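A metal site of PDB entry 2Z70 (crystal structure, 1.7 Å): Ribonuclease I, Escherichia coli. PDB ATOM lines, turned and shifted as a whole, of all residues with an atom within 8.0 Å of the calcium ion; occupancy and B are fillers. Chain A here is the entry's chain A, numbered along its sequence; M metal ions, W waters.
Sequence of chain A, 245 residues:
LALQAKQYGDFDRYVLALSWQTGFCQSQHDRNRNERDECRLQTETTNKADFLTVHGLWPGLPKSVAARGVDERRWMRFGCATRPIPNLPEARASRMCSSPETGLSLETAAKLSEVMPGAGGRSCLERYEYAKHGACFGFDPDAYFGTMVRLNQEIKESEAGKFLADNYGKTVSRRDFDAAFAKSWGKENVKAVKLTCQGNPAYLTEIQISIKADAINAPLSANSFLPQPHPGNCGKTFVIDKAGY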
ATOM      1  N   TRP A  20      18.335 -19.271 -26.627  1.00  0.00           N
ATOM      2  CA  TRP A  20      18.957 -18.159 -25.945  1.00  0.00           C
ATOM      3  C   TRP A  20      18.131 -18.082 -24.654  1.00  0.00           C
ATOM      4  O   TRP A  20      16.986 -17.610 -24.646  1.00  0.00           O
ATOM      5  CB  TRP A  20      18.862 -16.873 -26.784  1.00  0.00           C
ATOM      6  CG  TRP A  20      19.562 -15.745 -26.100  1.00  0.00           C
ATOM      7  CD1 TRP A  20      19.004 -14.562 -25.647  1.00  0.00           C
ATOM      8  CD2 TRP A  20      20.944 -15.723 -25.715  1.00  0.00           C
ATOM      9  NE1 TRP A  20      19.991 -13.787 -25.044  1.00  0.00           N
ATOM     10  CE2 TRP A  20      21.177 -14.478 -25.052  1.00  0.00           C
ATOM     11  CE3 TRP A  20      22.015 -16.615 -25.840  1.00  0.00           C
ATOM     12  CZ2 TRP A  20      22.430 -14.127 -24.523  1.00  0.00           C
ATOM     13  CZ3 TRP A  20      23.268 -16.244 -25.337  1.00  0.00           C
ATOM     14  CH2 TRP A  20      23.464 -15.018 -24.677  1.00  0.00           C
ATOM     15  N   GLN A  21      18.695 -18.624 -23.575  1.00  0.00           N
ATOM     16  CA  GLN A  21      17.883 -19.025 -22.402  1.00  0.00           C
ATOM     17  C   GLN A  21      17.166 -17.856 -21.766  1.00  0.00           C
ATOM     18  O   GLN A  21      16.022 -17.977 -21.360  1.00  0.00           O
ATOM     19  CB  GLN A  21      18.737 -19.759 -21.375  1.00  0.00           C
ATOM     20  CG  GLN A  21      17.940 -20.260 -20.170  1.00  0.00           C
ATOM     21  CD  GLN A  21      17.083 -21.442 -20.535  1.00  0.00           C
ATOM     22  OE1 GLN A  21      17.229 -22.028 -21.603  1.00  0.00           O
ATOM     23  NE2 GLN A  21      16.193 -21.818 -19.622  1.00  0.00           N
ATOM     24  N   THR A  22      17.834 -16.707 -21.739  1.00  0.00           N
ATOM     25  CA  THR A  22      17.238 -15.513 -21.172  1.00  0.00           C
ATOM     26  C   THR A  22      16.013 -15.109 -21.979  1.00  0.00           C
ATOM     27  O   THR A  22      14.966 -14.813 -21.406  1.00  0.00           O
ATOM     28  CB  THR A  22      18.253 -14.380 -21.073  1.00  0.00           C
ATOM     29  OG1 THR A  22      18.905 -14.227 -22.328  1.00  0.00           O
ATOM     30  CG2 THR A  22      19.321 -14.721 -19.997  1.00  0.00           C
ATOM     31  N   GLY A  23      16.142 -15.090 -23.310  1.00  0.00           N
ATOM     32  CA  GLY A  23      15.022 -14.780 -24.198  1.00  0.00           C
ATOM     33  C   GLY A  23      13.898 -15.820 -24.094  1.00  0.00           C
ATOM     34  O   GLY A  23      12.715 -15.463 -24.148  1.00  0.00           O
ATOM     35  N   PHE A  24      14.255 -17.092 -23.980  1.00  0.00           N
ATOM     36  CA  PHE A  24      13.241 -18.118 -23.794  1.00  0.00           C
ATOM     37  C   PHE A  24      12.396 -17.779 -22.556  1.00  0.00           C
ATOM     38  O   PHE A  24      11.175 -17.765 -22.612  1.00  0.00           O
ATOM     39  CB  PHE A  24      13.833 -19.519 -23.627  1.00  0.00           C
ATOM     40  CG  PHE A  24      12.839 -20.517 -23.091  1.00  0.00           C
ATOM     41  CD1 PHE A  24      11.803 -20.986 -23.890  1.00  0.00           C
ATOM     42  CD2 PHE A  24      12.902 -20.931 -21.765  1.00  0.00           C
ATOM     43  CE1 PHE A  24      10.850 -21.888 -23.388  1.00  0.00           C
ATOM     44  CE2 PHE A  24      11.971 -21.830 -21.242  1.00  0.00           C
ATOM     45  CZ  PHE A  24      10.942 -22.303 -22.063  1.00  0.00           C
ATOM     46  N   CYS A  25      13.081 -17.507 -21.441  1.00  0.00           N
ATOM     47  CA  CYS A  25      12.390 -17.198 -20.180  1.00  0.00           C
ATOM     48  C   CYS A  25      11.579 -15.915 -20.325  1.00  0.00           C
ATOM     49  O   CYS A  25      10.444 -15.829 -19.829  1.00  0.00           O
ATOM     50  CB  CYS A  25      13.384 -17.079 -19.028  1.00  0.00           C
ATOM     51  SG  CYS A  25      14.254 -18.633 -18.681  1.00  0.00           S
ATOM     52  N   GLN A  26      12.155 -14.931 -21.008  1.00  0.00           N
ATOM     53  CA  GLN A  26      11.489 -13.659 -21.269  1.00  0.00           C
ATOM     54  C   GLN A  26      10.181 -13.880 -22.017  1.00  0.00           C
ATOM     55  O   GLN A  26       9.155 -13.275 -21.682  1.00  0.00           O
ATOM     56  CB  GLN A  26      12.401 -12.710 -22.057  1.00  0.00           C
ATOM     57  CG  GLN A  26      11.801 -11.309 -22.264  1.00  0.00           C
ATOM     58  CD  GLN A  26      11.877 -10.454 -21.019  1.00  0.00           C
ATOM     59  OE1 GLN A  26      12.941 -10.308 -20.433  1.00  0.00           O
ATOM     60  NE2 GLN A  26      10.745  -9.858 -20.633  1.00  0.00           N
ATOM     61  N   SER A  27      10.219 -14.733 -23.040  1.00  0.00           N
ATOM     62  CA  SER A  27       9.047 -14.989 -23.889  1.00  0.00           C
ATOM     63  C   SER A  27       7.932 -15.699 -23.104  1.00  0.00           C
ATOM     64  O   SER A  27       6.748 -15.396 -23.300  1.00  0.00           O
ATOM     65  CB  SER A  27       9.423 -15.748 -25.165  1.00  0.00           C
ATOM     66  OG  SER A  27       9.766 -17.108 -24.884  1.00  0.00           O
ATOM     67  N   HIS A  29       7.427 -15.451 -19.855  1.00  0.00           N
ATOM     68  CA  HIS A  29       6.982 -14.358 -18.993  1.00  0.00           C
ATOM     69  C   HIS A  29       6.059 -13.403 -19.745  1.00  0.00           C
ATOM     70  O   HIS A  29       4.958 -13.118 -19.285  1.00  0.00           O
ATOM     71  CB  HIS A  29       8.186 -13.597 -18.438  1.00  0.00           C
ATOM     72  CG  HIS A  29       7.824 -12.431 -17.575  1.00  0.00           C
ATOM     73  ND1 HIS A  29       7.870 -11.125 -18.036  1.00  0.00           N
ATOM     74  CD2 HIS A  29       7.401 -12.362 -16.293  1.00  0.00           C
ATOM     75  CE1 HIS A  29       7.502 -10.310 -17.065  1.00  0.00           C
ATOM     76  NE2 HIS A  29       7.209 -11.040 -15.994  1.00  0.00           N
ATOM     77  N   ASP A  30       6.518 -12.902 -20.892  1.00  0.00           N
ATOM     78  CA  ASP A  30       5.732 -11.971 -21.722  1.00  0.00           C
ATOM     79  C   ASP A  30       4.355 -12.538 -22.126  1.00  0.00           C
ATOM     80  O   ASP A  30       3.394 -11.789 -22.285  1.00  0.00           O
ATOM     81  CB  ASP A  30       6.505 -11.585 -22.998  1.00  0.00           C
ATOM     82  CG  ASP A  30       7.683 -10.654 -22.726  1.00  0.00           C
ATOM     83  OD1 ASP A  30       7.883 -10.225 -21.572  1.00  0.00           O
ATOM     84  OD2 ASP A  30       8.425 -10.345 -23.690  1.00  0.00           O
ATOM     85  N   GLN A  42      16.299 -15.779 -12.588  1.00  0.00           N
ATOM     86  CA  GLN A  42      16.955 -14.943 -13.595  1.00  0.00           C
ATOM     87  C   GLN A  42      18.443 -14.807 -13.242  1.00  0.00           C
ATOM     88  O   GLN A  42      19.007 -13.704 -13.232  1.00  0.00           O
ATOM     89  CB  GLN A  42      16.279 -13.563 -13.693  1.00  0.00           C
ATOM     90  CG  GLN A  42      15.049 -13.509 -14.596  1.00  0.00           C
ATOM     91  CD  GLN A  42      14.142 -14.711 -14.475  1.00  0.00           C
ATOM     92  N   TYR A 168      25.871  -9.007 -25.361  1.00  0.00           N
ATOM     93  CA  TYR A 168      24.868  -9.312 -24.361  1.00  0.00           C
ATOM     94  C   TYR A 168      24.079  -8.048 -23.980  1.00  0.00           C
ATOM     95  O   TYR A 168      24.691  -7.027 -23.620  1.00  0.00           O
ATOM     96  CB  TYR A 168      25.549  -9.875 -23.135  1.00  0.00           C
ATOM     97  CG  TYR A 168      24.632 -10.221 -22.022  1.00  0.00           C
ATOM     98  CD1 TYR A 168      24.635  -9.473 -20.837  1.00  0.00           C
ATOM     99  CD2 TYR A 168      23.782 -11.317 -22.107  1.00  0.00           C
ATOM    100  CE1 TYR A 168      23.816  -9.798 -19.793  1.00  0.00           C
ATOM    101  CE2 TYR A 168      22.955 -11.648 -21.074  1.00  0.00           C
ATOM    102  CZ  TYR A 168      22.979 -10.889 -19.918  1.00  0.00           C
ATOM    103  OH  TYR A 168      22.159 -11.242 -18.879  1.00  0.00           O
ATOM    104  N   TYR A 203      13.484  -9.711 -29.446  1.00  0.00           N
ATOM    105  CA  TYR A 203      14.685 -10.254 -28.857  1.00  0.00           C
ATOM    106  C   TYR A 203      14.837 -11.717 -29.232  1.00  0.00           C
ATOM    107  O   TYR A 203      13.838 -12.406 -29.514  1.00  0.00           O
ATOM    108  CB  TYR A 203      14.674 -10.086 -27.331  1.00  0.00           C
ATOM    109  CG  TYR A 203      13.407 -10.656 -26.700  1.00  0.00           C
ATOM    110  CD1 TYR A 203      12.331  -9.838 -26.366  1.00  0.00           C
ATOM    111  CD2 TYR A 203      13.288 -12.014 -26.441  1.00  0.00           C
ATOM    112  CE1 TYR A 203      11.166 -10.344 -25.817  1.00  0.00           C
ATOM    113  CE2 TYR A 203      12.142 -12.545 -25.876  1.00  0.00           C
ATOM    114  CZ  TYR A 203      11.074 -11.700 -25.578  1.00  0.00           C
ATOM    115  OH  TYR A 203       9.936 -12.224 -25.012  1.00  0.00           O
ATOM    116  N   VAL A 239      17.353  -7.792 -30.264  1.00  0.00           N
ATOM    117  CA  VAL A 239      18.071  -7.630 -28.996  1.00  0.00           C
ATOM    118  C   VAL A 239      18.535  -8.970 -28.480  1.00  0.00           C
ATOM    119  O   VAL A 239      17.760  -9.954 -28.464  1.00  0.00           O
ATOM    120  CB  VAL A 239      17.141  -6.996 -27.916  1.00  0.00           C
ATOM    121  CG1 VAL A 239      17.843  -6.891 -26.567  1.00  0.00           C
ATOM    122  CG2 VAL A 239      16.660  -5.619 -28.354  1.00  0.00           C
ATOM    123  N   ILE A 240      19.774  -9.010 -28.012  1.00  0.00           N
ATOM    124  CA  ILE A 240      20.284 -10.186 -27.304  1.00  0.00           C
ATOM    125  C   ILE A 240      19.791 -10.076 -25.860  1.00  0.00           C
ATOM    126  O   ILE A 240      20.436  -9.418 -25.029  1.00  0.00           O
ATOM    127  CB  ILE A 240      21.847 -10.297 -27.405  1.00  0.00           C
ATOM    128  CG1 ILE A 240      22.312 -10.384 -28.884  1.00  0.00           C
ATOM    129  CG2 ILE A 240      22.350 -11.510 -26.611  1.00  0.00           C
ATOM    130  CD1 ILE A 240      21.565 -11.400 -29.729  1.00  0.00           C
ATOM    131  N   ASP A 241      18.645 -10.684 -25.585  1.00  0.00           N
ATOM    132  CA  ASP A 241      17.967 -10.518 -24.290  1.00  0.00           C
ATOM    133  C   ASP A 241      18.883 -10.748 -23.089  1.00  0.00           C
ATOM    134  O   ASP A 241      19.618 -11.739 -23.052  1.00  0.00           O
ATOM    135  CB  ASP A 241      16.751 -11.448 -24.195  1.00  0.00           C
ATOM    136  CG  ASP A 241      15.950 -11.199 -22.913  1.00  0.00           C
ATOM    137  OD1 ASP A 241      15.436 -10.066 -22.755  1.00  0.00           O
ATOM    138  OD2 ASP A 241      15.858 -12.109 -22.082  1.00  0.00           O
ATOM    139  N   LYS A 242      18.812  -9.832 -22.125  1.00  0.00           N
ATOM    140  CA  LYS A 242      19.509  -9.882 -20.835  1.00  0.00           C
ATOM    141  C   LYS A 242      18.688 -10.650 -19.812  1.00  0.00           C
ATOM    142  O   LYS A 242      17.456 -10.681 -19.896  1.00  0.00           O
ATOM    143  CB  LYS A 242      19.638  -8.453 -20.268  1.00  0.00           C
ATOM    144  CG  LYS A 242      20.924  -7.765 -20.522  1.00  0.00           C
ATOM    145  CD  LYS A 242      20.826  -6.352 -19.933  1.00  0.00           C
ATOM    146  N   ALA A 243      19.380 -11.246 -18.847  1.00  0.00           N
ATOM    147  CA  ALA A 243      18.725 -11.901 -17.725  1.00  0.00           C
ATOM    148  C   ALA A 243      17.905 -10.843 -16.995  1.00  0.00           C
ATOM    149  O   ALA A 243      18.305  -9.679 -16.940  1.00  0.00           O
ATOM    150  CB  ALA A 243      19.741 -12.529 -16.792  1.00  0.00           C
ATOM    151  N   GLY A 244      16.766 -11.268 -16.462  1.00  0.00           N
ATOM    152  CA  GLY A 244      15.797 -10.356 -15.858  1.00  0.00           C
ATOM    153  C   GLY A 244      14.651 -10.082 -16.813  1.00  0.00           C
ATOM    154  O   GLY A 244      14.823 -10.114 -18.043  1.00  0.00           O
ATOM    155  N   TYR A 245      13.460  -9.814 -16.263  1.00  0.00           N
ATOM    156  CA  TYR A 245      12.287  -9.572 -17.111  1.00  0.00           C
ATOM    157  C   TYR A 245      12.064  -8.096 -17.444  1.00  0.00           C
ATOM    158  O   TYR A 245      11.219  -7.732 -18.266  1.00  0.00           O
ATOM    159  CB  TYR A 245      11.036 -10.219 -16.505  1.00  0.00           C
ATOM    160  CG  TYR A 245      11.113 -11.734 -16.410  1.00  0.00           C
ATOM    161  CD1 TYR A 245      10.672 -12.393 -15.273  1.00  0.00           C
ATOM    162  CD2 TYR A 245      11.674 -12.502 -17.437  1.00  0.00           C
ATOM    163  CE1 TYR A 245      10.738 -13.773 -15.163  1.00  0.00           C
ATOM    164  CE2 TYR A 245      11.747 -13.874 -17.336  1.00  0.00           C
ATOM    165  CZ  TYR A 245      11.280 -14.503 -16.193  1.00  0.00           C
ATOM    166  OH  TYR A 245      11.334 -15.858 -16.058  1.00  0.00           O
ATOM    167  OXT TYR A 245      12.757  -7.229 -16.911  1.00  0.00           O
HETATM  168 CA    CA M   1      15.165 -10.612 -20.298  1.00  0.00          CA
HETATM  169  O   HOH W   1      15.529  -8.243 -20.355  1.00  0.00           O
HETATM  170  O   HOH W   2      14.925 -12.757 -19.469  1.00  0.00           O
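O of Asp 241 lies within hydrogen-bond range of OG1 of Thr 22 (2.7 Å).
The chain-end carboxylate (O) of Tyr 245 sits at hydrogen-bond distance from the side-chain amide nitrogen (NE2) of Gln 26, at 3.2 Å.
The side-chain carboxylate of Asp 241 lies close to the backbone NH of Gly 23 (3.2 Å).
The side-chain amide nitrogen (NE2) of Gln 26 lies within hydrogen-bond range of the side-chain carboxylate (OD1) of Asp 30.
O of Asp 241 lies within hydrogen-bond range of NE1 of Trp 20.
Within 4 Å of the calcium ion: Gln 26, Asp 241, Lys 242 and Gly 244.
The nearest printed residue that does not touch the calcium ion is Ala 243 (4.3 Å).
The calcium ion is bound by the side-chain amide oxygen (OE1) of Gln 26, at 2.2 Å.
Water W2 is bound to the calcium ion.
The backbone carbonyl oxygen (O) of Lys 242 binds the calcium ion.
O of Gly 244 is bound to the calcium ion (2.3 Å).
Water W1 is bound to the calcium ion (2.4 Å).
The calcium ion is bound by OD2 of Asp 241 (2.4 Å).
The calcium ion is bound by OD1 of Asp 241, 2.5 Å away.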
